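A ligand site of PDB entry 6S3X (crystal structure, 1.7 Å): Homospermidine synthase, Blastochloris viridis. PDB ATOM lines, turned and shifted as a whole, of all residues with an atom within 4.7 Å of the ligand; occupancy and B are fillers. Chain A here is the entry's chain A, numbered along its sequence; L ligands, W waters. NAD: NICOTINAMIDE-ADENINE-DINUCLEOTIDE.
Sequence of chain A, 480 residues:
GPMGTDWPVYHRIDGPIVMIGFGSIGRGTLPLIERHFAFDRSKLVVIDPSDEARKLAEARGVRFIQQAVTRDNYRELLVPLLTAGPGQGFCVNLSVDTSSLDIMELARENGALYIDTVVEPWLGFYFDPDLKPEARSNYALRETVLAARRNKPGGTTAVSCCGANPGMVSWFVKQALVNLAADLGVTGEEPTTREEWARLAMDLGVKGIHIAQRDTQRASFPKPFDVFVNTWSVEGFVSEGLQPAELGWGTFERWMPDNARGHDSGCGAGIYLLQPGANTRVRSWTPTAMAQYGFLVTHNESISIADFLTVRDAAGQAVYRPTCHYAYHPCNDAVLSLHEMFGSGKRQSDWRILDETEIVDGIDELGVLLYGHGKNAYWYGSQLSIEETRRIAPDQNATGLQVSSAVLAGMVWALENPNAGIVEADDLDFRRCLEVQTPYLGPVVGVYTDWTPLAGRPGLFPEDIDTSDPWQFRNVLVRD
O of Val 69 is in hydrogen-bond range of N6A of the ligand, at 2.9 Å. The side-chain hydroxyl of Thr 117 is in hydrogen-bond range of an oxygen (O4D) of the ligand, 3.0 Å away. O of Asn 165 is in hydrogen-bond range of N7N of the ligand (3.2 Å). N of Ile 25 lies within hydrogen-bond range of O2N of the ligand (2.9 Å). The side-chain hydroxyl (OG) of Ser 233 lies within hydrogen-bond range of an oxygen (O2A) of the ligand (2.9 Å). O1A of the ligand is in hydrogen-bond range of N of Ser 24 (3.0 Å). The backbone NH (N) of Ser 233 is in hydrogen-bond range of an oxygen (O1N) of the ligand (3.0 Å). The backbone carbonyl oxygen of Ser 95 lies within hydrogen-bond range of an oxygen (O3D) of the ligand (2.8 Å). O3B of the ligand is in hydrogen-bond range of OD2 of Asp 48 (2.6 Å). An oxygen (O1N) of the ligand sits at hydrogen-bond distance from the side-chain hydroxyl of Ser 24, at 2.7 Å. The backbone NH of Val 69 is in hydrogen-bond range of a nitrogen (N1A) of the ligand (3.1 Å).
Water W2 lies within hydrogen-bond range of the backbone carbonyl oxygen (O) of Leu 94 (2.7 Å), an oxygen (O2N) of the ligand (2.7 Å), the backbone NH (N) of Gly 23 (3.0 Å) and the backbone NH (N) of Gly 26 (3.0 Å). Water W1 bridges OD2 of Asp 97 (2.8 Å) and N7A of the ligand (2.8 Å). Water W8 bridges OE1 of Glu 120 (2.7 Å) and O2D of the ligand (2.9 Å). Water W7 lies within hydrogen-bond range of an oxygen (O2A) of the ligand and the side-chain hydroxyl (OG) of Ser 233.
N of Phe 22 sits at hydrogen-bond distance from OD2 of Asp 48, 2.8 Å away. The backbone carbonyl oxygen of Gly 23 sits close to the guanidinium group of Arg 27 (3.2 Å). The backbone NH (N) of Leu 94 sits at hydrogen-bond distance from the backbone carbonyl oxygen (O) of Ile 20, at 2.8 Å. The backbone carbonyl oxygen (O) of Ile 20 is in hydrogen-bond range of the backbone NH (N) of Ser 95 (3.4 Å). The backbone carbonyl oxygen (O) of Phe 22 lies within hydrogen-bond range of the guanidinium group (NE) of Arg 27, 2.8 Å away. OG1 of Thr 98 sits at hydrogen-bond distance from OG of Ser 95, 2.5 Å away. The side-chain carboxylate (OD1) of Asp 48 lies within hydrogen-bond range of the backbone NH (N) of Ser 50, at 2.8 Å. The backbone NH of Gly 236 is in hydrogen-bond range of the side-chain hydroxyl of Ser 233, 2.7 Å away.
N7A of the ligand sits close to O of Val 96, at 3.3 Å. A nitrogen (N7N) of the ligand sits close to the backbone NH (N) of Ala 164 (2.9 Å). O of Pro 166 lies close to O7N of the ligand (3.3 Å). CG2 of Ile 20 touches C2A of the ligand (3.9 Å). Phe 22 touches the ligand. Gly 23 touches the ligand (CA to O5B, 3.5 Å). Pro 49 touches the ligand (CD to C4A, 3.3 Å). CB of Ser 50 touches O2B of the ligand (3.95 Å). CB of Ala 68 touches N6A of the ligand, at 3.4 Å. Leu 94 touches the ligand. CG2 of Thr 98 touches N1A of the ligand, at 3.6 Å. CG1 of Val 118 touches O3D of the ligand, 3.5 Å away. Gly 163 touches the ligand. CE3 of Trp 232 touches C5N of the ligand, at 3.6 Å. Ile 353 touches the ligand (CD1 to O1A, 3.5 Å). CG2 of Val 403 touches C4N of the ligand, 3.4 Å away. Hydrophobic or aromatic side chains within 4 Å of the ligand: Ile 20, Ile 25, Pro 49, Ala 68, Val 69, Val 96, Val 118, Ala 164, Pro 166, Trp 232, Ile 353 and Val 403. Within 4 Å of the ligand: Ile 20, Phe 22, Gly 23, Ser 24, Ile 25, Asp 48, Pro 49, Ser 50, Ala 68, Val 69, Leu 94, Ser 95, Val 96, Thr 98, Thr 117, Val 118, Gly 163, Ala 164, Asn 165, Pro 166, Trp 232, Ser 233, Ile 353 and Val 403. The nearest printed residue that does not touch the ligand is Gly 21 (4.01 Å).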
ATOM      1  N   ILE A  20     -26.819   5.085  11.410  1.00  0.00           N
ATOM      2  CA  ILE A  20     -28.068   4.702  12.045  1.00  0.00           C
ATOM      3  C   ILE A  20     -27.801   4.635  13.539  1.00  0.00           C
ATOM      4  O   ILE A  20     -26.973   3.834  13.979  1.00  0.00           O
ATOM      5  CB  ILE A  20     -28.580   3.363  11.500  1.00  0.00           C
ATOM      6  CG1 ILE A  20     -28.700   3.429   9.970  1.00  0.00           C
ATOM      7  CG2 ILE A  20     -29.890   2.997  12.123  1.00  0.00           C
ATOM      8  CD1 ILE A  20     -29.097   2.108   9.336  1.00  0.00           C
ATOM      9  N   GLY A  21     -28.456   5.496  14.310  1.00  0.00           N
ATOM     10  CA  GLY A  21     -28.212   5.583  15.732  1.00  0.00           C
ATOM     11  C   GLY A  21     -27.178   6.632  16.070  1.00  0.00           C
ATOM     12  O   GLY A  21     -26.087   6.648  15.483  1.00  0.00           O
ATOM     13  N   PHE A  22     -27.503   7.528  16.991  1.00  0.00           N
ATOM     14  CA  PHE A  22     -26.572   8.572  17.381  1.00  0.00           C
ATOM     15  C   PHE A  22     -26.601   8.700  18.903  1.00  0.00           C
ATOM     16  O   PHE A  22     -26.905   9.742  19.478  1.00  0.00           O
ATOM     17  CB  PHE A  22     -26.918   9.881  16.665  1.00  0.00           C
ATOM     18  CG  PHE A  22     -25.776  10.841  16.639  1.00  0.00           C
ATOM     19  CD1 PHE A  22     -24.612  10.532  15.962  1.00  0.00           C
ATOM     20  CD2 PHE A  22     -25.870  12.041  17.304  1.00  0.00           C
ATOM     21  CE1 PHE A  22     -23.557  11.397  15.956  1.00  0.00           C
ATOM     22  CE2 PHE A  22     -24.809  12.929  17.288  1.00  0.00           C
ATOM     23  CZ  PHE A  22     -23.642  12.601  16.625  1.00  0.00           C
ATOM     24  N   GLY A  23     -26.285   7.597  19.566  1.00  0.00           N
ATOM     25  CA  GLY A  23     -26.124   7.523  21.013  1.00  0.00           C
ATOM     26  C   GLY A  23     -24.677   7.659  21.408  1.00  0.00           C
ATOM     27  O   GLY A  23     -23.899   8.372  20.774  1.00  0.00           O
ATOM     28  N   SER A  24     -24.286   6.936  22.462  1.00  0.00           N
ATOM     29  CA  SER A  24     -22.948   7.144  23.005  1.00  0.00           C
ATOM     30  C   SER A  24     -21.868   6.767  22.005  1.00  0.00           C
ATOM     31  O   SER A  24     -20.874   7.484  21.856  1.00  0.00           O
ATOM     32  CB  SER A  24     -22.793   6.401  24.343  1.00  0.00           C
ATOM     33  OG  SER A  24     -22.349   5.077  24.199  1.00  0.00           O
ATOM     34  N   ILE A  25     -22.061   5.677  21.243  1.00  0.00           N
ATOM     35  CA  ILE A  25     -21.020   5.265  20.310  1.00  0.00           C
ATOM     36  C   ILE A  25     -21.072   6.106  19.017  1.00  0.00           C
ATOM     37  O   ILE A  25     -20.030   6.529  18.517  1.00  0.00           O
ATOM     38  CB  ILE A  25     -21.133   3.762  20.004  1.00  0.00           C
ATOM     39  CG1 ILE A  25     -21.043   2.928  21.284  1.00  0.00           C
ATOM     40  CG2 ILE A  25     -20.056   3.326  19.038  1.00  0.00           C
ATOM     41  CD1 ILE A  25     -19.845   3.239  22.147  1.00  0.00           C
ATOM     42  N   GLY A  26     -22.269   6.380  18.486  1.00  0.00           N
ATOM     43  CA  GLY A  26     -22.350   7.239  17.319  1.00  0.00           C
ATOM     44  C   GLY A  26     -21.743   8.596  17.555  1.00  0.00           C
ATOM     45  O   GLY A  26     -21.064   9.138  16.674  1.00  0.00           O
ATOM     46  N   ARG A  27     -21.953   9.164  18.742  1.00  0.00           N
ATOM     47  CA  ARG A  27     -21.371  10.454  19.098  1.00  0.00           C
ATOM     48  C   ARG A  27     -19.853  10.403  19.119  1.00  0.00           C
ATOM     49  O   ARG A  27     -19.182  11.384  18.785  1.00  0.00           O
ATOM     50  CB  ARG A  27     -21.892  10.901  20.467  1.00  0.00           C
ATOM     51  CG  ARG A  27     -23.324  11.372  20.456  1.00  0.00           C
ATOM     52  CD  ARG A  27     -24.067  11.239  21.772  1.00  0.00           C
ATOM     53  NE  ARG A  27     -25.491  11.050  21.480  1.00  0.00           N
ATOM     54  CZ  ARG A  27     -26.485  11.171  22.352  1.00  0.00           C
ATOM     55  NH1 ARG A  27     -26.240  11.476  23.614  1.00  0.00           N
ATOM     56  NH2 ARG A  27     -27.729  10.975  21.953  1.00  0.00           N
ATOM     57  N   ILE A  47     -29.564   9.090  11.346  1.00  0.00           N
ATOM     58  CA  ILE A  47     -30.951   8.688  11.572  1.00  0.00           C
ATOM     59  C   ILE A  47     -31.088   8.225  13.006  1.00  0.00           C
ATOM     60  O   ILE A  47     -30.428   7.255  13.405  1.00  0.00           O
ATOM     61  CB  ILE A  47     -31.374   7.552  10.633  1.00  0.00           C
ATOM     62  CG1 ILE A  47     -31.049   7.876   9.177  1.00  0.00           C
ATOM     63  CG2 ILE A  47     -32.840   7.238  10.794  1.00  0.00           C
ATOM     64  CD1 ILE A  47     -31.228   6.689   8.294  1.00  0.00           C
ATOM     65  N   ASP A  48     -31.964   8.861  13.775  1.00  0.00           N
ATOM     66  CA  ASP A  48     -32.201   8.487  15.165  1.00  0.00           C
ATOM     67  C   ASP A  48     -33.564   9.015  15.576  1.00  0.00           C
ATOM     68  O   ASP A  48     -33.892  10.160  15.239  1.00  0.00           O
ATOM     69  CB  ASP A  48     -31.104   9.058  16.082  1.00  0.00           C
ATOM     70  CG  ASP A  48     -31.123   8.470  17.504  1.00  0.00           C
ATOM     71  OD1 ASP A  48     -32.149   8.619  18.208  1.00  0.00           O
ATOM     72  OD2 ASP A  48     -30.099   7.888  17.927  1.00  0.00           O
ATOM     73  N   PRO A  49     -34.376   8.230  16.302  1.00  0.00           N
ATOM     74  CA  PRO A  49     -35.685   8.743  16.712  1.00  0.00           C
ATOM     75  C   PRO A  49     -35.665   9.801  17.810  1.00  0.00           C
ATOM     76  O   PRO A  49     -36.706  10.435  18.032  1.00  0.00           O
ATOM     77  CB  PRO A  49     -36.429   7.475  17.197  1.00  0.00           C
ATOM     78  CG  PRO A  49     -35.309   6.584  17.701  1.00  0.00           C
ATOM     79  CD  PRO A  49     -34.154   6.842  16.740  1.00  0.00           C
ATOM     80  N   SER A  50     -34.542  10.045  18.484  1.00  0.00           N
ATOM     81  CA  SER A  50     -34.626  10.837  19.704  1.00  0.00           C
ATOM     82  C   SER A  50     -34.341  12.335  19.472  1.00  0.00           C
ATOM     83  O   SER A  50     -33.570  12.713  18.596  1.00  0.00           O
ATOM     84  CB  SER A  50     -33.654  10.311  20.769  1.00  0.00           C
ATOM     85  OG  SER A  50     -32.342  10.832  20.571  1.00  0.00           O
ATOM     86  N   GLN A  67     -36.287   9.540  12.746  1.00  0.00           N
ATOM     87  CA  GLN A  67     -37.099   8.358  12.564  1.00  0.00           C
ATOM     88  C   GLN A  67     -36.451   7.196  13.306  1.00  0.00           C
ATOM     89  O   GLN A  67     -35.218   7.123  13.432  1.00  0.00           O
ATOM     90  CB  GLN A  67     -37.232   7.948  11.097  1.00  0.00           C
ATOM     91  CG  GLN A  67     -38.006   8.938  10.223  1.00  0.00           C
ATOM     92  CD  GLN A  67     -39.480   8.937  10.549  1.00  0.00           C
ATOM     93  OE1 GLN A  67     -40.004   7.967  11.096  1.00  0.00           O
ATOM     94  NE2 GLN A  67     -40.154  10.033  10.218  1.00  0.00           N
ATOM     95  N   ALA A  68     -37.293   6.300  13.810  1.00  0.00           N
ATOM     96  CA  ALA A  68     -36.846   4.978  14.209  1.00  0.00           C
ATOM     97  C   ALA A  68     -36.899   4.093  12.966  1.00  0.00           C
ATOM     98  O   ALA A  68     -37.903   4.084  12.247  1.00  0.00           O
ATOM     99  CB  ALA A  68     -37.713   4.406  15.328  1.00  0.00           C
ATOM    100  N   VAL A  69     -35.806   3.389  12.695  1.00  0.00           N
ATOM    101  CA  VAL A  69     -35.766   2.381  11.652  1.00  0.00           C
ATOM    102  C   VAL A  69     -36.488   1.137  12.168  1.00  0.00           C
ATOM    103  O   VAL A  69     -36.140   0.619  13.227  1.00  0.00           O
ATOM    104  CB  VAL A  69     -34.328   2.059  11.243  1.00  0.00           C
ATOM    105  CG1 VAL A  69     -34.294   1.010  10.172  1.00  0.00           C
ATOM    106  CG2 VAL A  69     -33.636   3.325  10.772  1.00  0.00           C
ATOM    107  N   LEU A  94     -25.025   1.847  14.444  1.00  0.00           N
ATOM    108  CA  LEU A  94     -24.670   1.962  15.854  1.00  0.00           C
ATOM    109  C   LEU A  94     -25.910   2.177  16.685  1.00  0.00           C
ATOM    110  O   LEU A  94     -25.978   3.021  17.581  1.00  0.00           O
ATOM    111  CB  LEU A  94     -23.705   3.106  16.073  1.00  0.00           C
ATOM    112  CG  LEU A  94     -22.475   3.013  15.175  1.00  0.00           C
ATOM    113  CD1 LEU A  94     -21.685   4.272  15.331  1.00  0.00           C
ATOM    114  CD2 LEU A  94     -21.676   1.786  15.563  1.00  0.00           C
ATOM    115  N   SER A  95     -26.928   1.383  16.383  1.00  0.00           N
ATOM    116  CA  SER A  95     -28.257   1.567  16.914  1.00  0.00           C
ATOM    117  C   SER A  95     -28.623   0.449  17.885  1.00  0.00           C
ATOM    118  O   SER A  95     -27.891  -0.536  18.033  1.00  0.00           O
ATOM    119  CB  SER A  95     -29.285   1.626  15.767  1.00  0.00           C
ATOM    120  OG  SER A  95     -29.337   0.383  15.073  1.00  0.00           O
ATOM    121  N   VAL A  96     -29.759   0.629  18.543  1.00  0.00           N
ATOM    122  CA  VAL A  96     -30.459  -0.473  19.190  1.00  0.00           C
ATOM    123  C   VAL A  96     -31.786  -0.683  18.467  1.00  0.00           C
ATOM    124  O   VAL A  96     -32.256   0.155  17.715  1.00  0.00           O
ATOM    125  CB  VAL A  96     -30.694  -0.268  20.703  1.00  0.00           C
ATOM    126  CG1 VAL A  96     -29.372  -0.176  21.445  1.00  0.00           C
ATOM    127  CG2 VAL A  96     -31.576   0.959  20.975  1.00  0.00           C
ATOM    128  N   ASP A  97     -32.379  -1.845  18.721  1.00  0.00           N
ATOM    129  CA  ASP A  97     -33.744  -2.181  18.308  1.00  0.00           C
ATOM    130  C   ASP A  97     -33.905  -2.331  16.788  1.00  0.00           C
ATOM    131  O   ASP A  97     -35.033  -2.352  16.305  1.00  0.00           O
ATOM    132  CB  ASP A  97     -34.751  -1.146  18.807  1.00  0.00           C
ATOM    133  CG  ASP A  97     -34.866  -1.132  20.313  1.00  0.00           C
ATOM    134  OD1 ASP A  97     -34.475  -2.131  20.948  1.00  0.00           O
ATOM    135  OD2 ASP A  97     -35.348  -0.117  20.864  1.00  0.00           O
ATOM    136  N   THR A  98     -32.808  -2.436  16.040  1.00  0.00           N
ATOM    137  CA  THR A  98     -32.865  -2.638  14.599  1.00  0.00           C
ATOM    138  C   THR A  98     -32.243  -3.995  14.271  1.00  0.00           C
ATOM    139  O   THR A  98     -31.335  -4.464  14.977  1.00  0.00           O
ATOM    140  CB  THR A  98     -32.098  -1.552  13.868  1.00  0.00           C
ATOM    141  OG1 THR A  98     -30.732  -1.571  14.305  1.00  0.00           O
ATOM    142  CG2 THR A  98     -32.678  -0.178  14.166  1.00  0.00           C
ATOM    143  N   THR A 117     -21.719  -3.301  15.427  1.00  0.00           N
ATOM    144  CA  THR A 117     -20.991  -3.734  16.606  1.00  0.00           C
ATOM    145  C   THR A 117     -21.736  -4.801  17.401  1.00  0.00           C
ATOM    146  O   THR A 117     -21.329  -5.118  18.528  1.00  0.00           O
ATOM    147  CB  THR A 117     -20.705  -2.535  17.527  1.00  0.00           C
ATOM    148  OG1 THR A 117     -21.949  -2.038  18.046  1.00  0.00           O
ATOM    149  CG2 THR A 117     -20.006  -1.430  16.749  1.00  0.00           C
ATOM    150  N   VAL A 118     -22.794  -5.361  16.858  1.00  0.00           N
ATOM    151  CA  VAL A 118     -23.666  -6.273  17.576  1.00  0.00           C
ATOM    152  C   VAL A 118     -24.560  -6.895  16.515  1.00  0.00           C
ATOM    153  O   VAL A 118     -24.869  -6.249  15.509  1.00  0.00           O
ATOM    154  CB  VAL A 118     -24.487  -5.548  18.664  1.00  0.00           C
ATOM    155  CG1 VAL A 118     -25.384  -4.466  18.056  1.00  0.00           C
ATOM    156  CG2 VAL A 118     -25.264  -6.550  19.495  1.00  0.00           C
ATOM    157  N   GLU A 120     -28.010  -7.345  16.348  1.00  0.00           N
ATOM    158  CA  GLU A 120     -29.222  -6.896  16.998  1.00  0.00           C
ATOM    159  C   GLU A 120     -30.427  -7.365  16.224  1.00  0.00           C
ATOM    160  O   GLU A 120     -30.389  -7.434  14.995  1.00  0.00           O
ATOM    161  CB  GLU A 120     -29.189  -5.375  17.098  1.00  0.00           C
ATOM    162  CG  GLU A 120     -30.337  -4.713  17.849  1.00  0.00           C
ATOM    163  CD  GLU A 120     -30.118  -4.617  19.345  1.00  0.00           C
ATOM    164  OE1 GLU A 120     -29.167  -5.229  19.856  1.00  0.00           O
ATOM    165  OE2 GLU A 120     -30.910  -3.917  20.024  1.00  0.00           O
ATOM    166  N   GLY A 163     -16.901  -3.816  17.164  1.00  0.00           N
ATOM    167  CA  GLY A 163     -16.616  -2.830  18.187  1.00  0.00           C
ATOM    168  C   GLY A 163     -15.382  -3.150  18.996  1.00  0.00           C
ATOM    169  O   GLY A 163     -14.399  -3.685  18.468  1.00  0.00           O
ATOM    170  N   ALA A 164     -15.406  -2.837  20.302  1.00  0.00           N
ATOM    171  CA  ALA A 164     -14.304  -3.207  21.189  1.00  0.00           C
ATOM    172  C   ALA A 164     -14.356  -4.674  21.554  1.00  0.00           C
ATOM    173  O   ALA A 164     -13.329  -5.370  21.554  1.00  0.00           O
ATOM    174  CB  ALA A 164     -14.338  -2.345  22.439  1.00  0.00           C
ATOM    175  N   ASN A 165     -15.545  -5.160  21.891  1.00  0.00           N
ATOM    176  CA  ASN A 165     -15.792  -6.559  22.231  1.00  0.00           C
ATOM    177  C   ASN A 165     -17.296  -6.780  22.121  1.00  0.00           C
ATOM    178  O   ASN A 165     -18.063  -6.335  22.989  1.00  0.00           O
ATOM    179  CB  ASN A 165     -15.261  -6.899  23.629  1.00  0.00           C
ATOM    180  CG  ASN A 165     -15.785  -5.989  24.719  1.00  0.00           C
ATOM    181  OD1 ASN A 165     -15.820  -4.762  24.569  1.00  0.00           O
ATOM    182  ND2 ASN A 165     -16.159  -6.584  25.835  1.00  0.00           N
ATOM    183  N   PRO A 166     -17.766  -7.465  21.068  1.00  0.00           N
ATOM    184  CA  PRO A 166     -16.951  -8.062  20.001  1.00  0.00           C
ATOM    185  C   PRO A 166     -16.232  -7.056  19.114  1.00  0.00           C
ATOM    186  O   PRO A 166     -16.656  -5.900  19.033  1.00  0.00           O
ATOM    187  CB  PRO A 166     -17.987  -8.859  19.189  1.00  0.00           C
ATOM    188  CG  PRO A 166     -19.282  -8.108  19.419  1.00  0.00           C
ATOM    189  CD  PRO A 166     -19.212  -7.687  20.859  1.00  0.00           C
ATOM    190  N   TRP A 232     -21.816   2.994  28.813  1.00  0.00           N
ATOM    191  CA  TRP A 232     -22.298   2.845  27.456  1.00  0.00           C
ATOM    192  C   TRP A 232     -23.757   2.431  27.565  1.00  0.00           C
ATOM    193  O   TRP A 232     -24.305   2.326  28.680  1.00  0.00           O
ATOM    194  CB  TRP A 232     -21.423   1.854  26.686  1.00  0.00           C
ATOM    195  CG  TRP A 232     -21.445   0.475  27.293  1.00  0.00           C
ATOM    196  CD1 TRP A 232     -20.768   0.049  28.396  1.00  0.00           C
ATOM    197  CD2 TRP A 232     -22.190  -0.632  26.811  1.00  0.00           C
ATOM    198  NE1 TRP A 232     -21.047  -1.277  28.633  1.00  0.00           N
ATOM    199  CE2 TRP A 232     -21.918  -1.723  27.667  1.00  0.00           C
ATOM    200  CE3 TRP A 232     -23.062  -0.822  25.733  1.00  0.00           C
ATOM    201  CZ2 TRP A 232     -22.494  -2.980  27.477  1.00  0.00           C
ATOM    202  CZ3 TRP A 232     -23.620  -2.066  25.542  1.00  0.00           C
ATOM    203  CH2 TRP A 232     -23.337  -3.124  26.422  1.00  0.00           C
ATOM    204  N   SER A 233     -24.390   2.181  26.405  1.00  0.00           N
ATOM    205  CA  SER A 233     -25.811   1.860  26.365  1.00  0.00           C
ATOM    206  C   SER A 233     -26.332   1.131  27.597  1.00  0.00           C
ATOM    207  O   SER A 233     -25.864   0.035  27.918  1.00  0.00           O
ATOM    208  CB  SER A 233     -26.136   0.978  25.149  1.00  0.00           C
ATOM    209  OG  SER A 233     -27.543   0.889  24.961  1.00  0.00           O
ATOM    210  N   GLY A 236     -28.760  -1.417  25.788  1.00  0.00           N
ATOM    211  CA  GLY A 236     -28.009  -2.517  25.215  1.00  0.00           C
ATOM    212  C   GLY A 236     -27.429  -3.452  26.260  1.00  0.00           C
ATOM    213  O   GLY A 236     -27.429  -4.678  26.092  1.00  0.00           O
ATOM    214  N   ILE A 353     -26.201   7.338  31.014  1.00  0.00           N
ATOM    215  CA  ILE A 353     -24.888   6.973  30.531  1.00  0.00           C
ATOM    216  C   ILE A 353     -23.918   8.073  30.939  1.00  0.00           C
ATOM    217  O   ILE A 353     -24.133   9.251  30.606  1.00  0.00           O
ATOM    218  CB  ILE A 353     -24.891   6.782  29.011  1.00  0.00           C
ATOM    219  CG1 ILE A 353     -25.815   5.639  28.595  1.00  0.00           C
ATOM    220  CG2 ILE A 353     -23.452   6.572  28.518  1.00  0.00           C
ATOM    221  CD1 ILE A 353     -26.033   5.547  27.066  1.00  0.00           C
ATOM    222  N   VAL A 403     -14.510   1.444  21.458  1.00  0.00           N
ATOM    223  CA  VAL A 403     -15.492   0.970  20.478  1.00  0.00           C
ATOM    224  C   VAL A 403     -15.403   1.764  19.178  1.00  0.00           C
ATOM    225  O   VAL A 403     -15.296   1.192  18.092  1.00  0.00           O
ATOM    226  CB  VAL A 403     -16.898   1.035  21.088  1.00  0.00           C
ATOM    227  CG1 VAL A 403     -17.951   0.575  20.069  1.00  0.00           C
ATOM    228  CG2 VAL A 403     -16.972   0.220  22.401  1.00  0.00           C
HETATM  229  PA  NAD L   1     -27.134   4.073  23.156  1.00  0.00           P
HETATM  230  O1A NAD L   1     -26.399   5.147  23.640  1.00  0.00           O
HETATM  231  O2A NAD L   1     -28.185   3.551  23.928  1.00  0.00           O
HETATM  232  O5B NAD L   1     -27.690   4.529  21.781  1.00  0.00           O
HETATM  233  C5B NAD L   1     -28.604   3.794  21.029  1.00  0.00           C
HETATM  234  C4B NAD L   1     -29.227   4.754  20.005  1.00  0.00           C
HETATM  235  O4B NAD L   1     -30.067   4.108  19.107  1.00  0.00           O
HETATM  236  C3B NAD L   1     -30.088   5.799  20.692  1.00  0.00           C
HETATM  237  O3B NAD L   1     -29.660   7.110  20.374  1.00  0.00           O
HETATM  238  C2B NAD L   1     -31.510   5.527  20.214  1.00  0.00           C
HETATM  239  O2B NAD L   1     -32.326   6.652  20.093  1.00  0.00           O
HETATM  240  C1B NAD L   1     -31.213   4.888  18.899  1.00  0.00           C
HETATM  241  N9A NAD L   1     -32.337   4.096  18.436  1.00  0.00           N
HETATM  242  C8A NAD L   1     -33.234   3.450  19.141  1.00  0.00           C
HETATM  243  N7A NAD L   1     -34.086   2.829  18.353  1.00  0.00           N
HETATM  244  C5A NAD L   1     -33.744   3.099  17.118  1.00  0.00           C
HETATM  245  C6A NAD L   1     -34.209   2.778  15.784  1.00  0.00           C
HETATM  246  N6A NAD L   1     -35.278   2.002  15.630  1.00  0.00           N
HETATM  247  N1A NAD L   1     -33.512   3.264  14.785  1.00  0.00           N
HETATM  248  C2A NAD L   1     -32.473   4.012  14.929  1.00  0.00           C
HETATM  249  N3A NAD L   1     -32.011   4.359  16.087  1.00  0.00           N
HETATM  250  C4A NAD L   1     -32.583   3.942  17.187  1.00  0.00           C
HETATM  251  O3  NAD L   1     -26.190   2.920  22.727  1.00  0.00           O
HETATM  252  PN  NAD L   1     -24.678   2.970  22.402  1.00  0.00           P
HETATM  253  O1N NAD L   1     -23.911   2.971  23.580  1.00  0.00           O
HETATM  254  O2N NAD L   1     -24.343   3.954  21.448  1.00  0.00           O
HETATM  255  O5D NAD L   1     -24.465   1.597  21.742  1.00  0.00           O
HETATM  256  C5D NAD L   1     -25.040   1.400  20.506  1.00  0.00           C
HETATM  257  C4D NAD L   1     -24.993  -0.023  20.002  1.00  0.00           C
HETATM  258  O4D NAD L   1     -23.677  -0.533  19.967  1.00  0.00           O
HETATM  259  C3D NAD L   1     -25.792  -0.927  20.893  1.00  0.00           C
HETATM  260  O3D NAD L   1     -26.510  -1.846  20.091  1.00  0.00           O
HETATM  261  C2D NAD L   1     -24.720  -1.596  21.713  1.00  0.00           C
HETATM  262  O2D NAD L   1     -25.109  -2.884  22.160  1.00  0.00           O
HETATM  263  C1D NAD L   1     -23.559  -1.696  20.738  1.00  0.00           C
HETATM  264  N1N NAD L   1     -22.264  -1.694  21.393  1.00  0.00           N
HETATM  265  C2N NAD L   1     -21.318  -2.544  21.063  1.00  0.00           C
HETATM  266  C3N NAD L   1     -20.094  -2.530  21.678  1.00  0.00           C
HETATM  267  C7N NAD L   1     -18.999  -3.473  21.265  1.00  0.00           C
HETATM  268  O7N NAD L   1     -19.151  -4.265  20.390  1.00  0.00           O
HETATM  269  N7N NAD L   1     -17.837  -3.364  21.822  1.00  0.00           N
HETATM  270  C4N NAD L   1     -19.865  -1.608  22.651  1.00  0.00           C
HETATM  271  C5N NAD L   1     -20.842  -0.708  22.947  1.00  0.00           C
HETATM  272  C6N NAD L   1     -22.027  -0.789  22.284  1.00  0.00           C
HETATM  273  O   HOH W   1     -36.539   1.718  19.167  1.00  0.00           O
HETATM  274  O   HOH W   2     -24.868   5.064  19.009  1.00  0.00           O
HETATM  275  O   HOH W   3     -34.259   6.601  21.886  1.00  0.00           O
HETATM  276  O   HOH W   4     -27.178   7.744  24.552  1.00  0.00           O
HETATM  277  O   HOH W   5     -30.842   4.141  23.569  1.00  0.00           O
HETATM  278  O   HOH W   6     -33.949   3.122  22.237  1.00  0.00           O
HETATM  279  O   HOH W   7     -29.144   3.365  26.749  1.00  0.00           O
HETATM  280  O   HOH W   8     -27.723  -3.987  21.748  1.00  0.00           O
HETATM  281  O   HOH W   9     -37.769   0.994  17.141  1.00  0.00           O
HETATM  282  O   HOH W  10     -23.106  -4.928  22.898  1.00  0.00           O
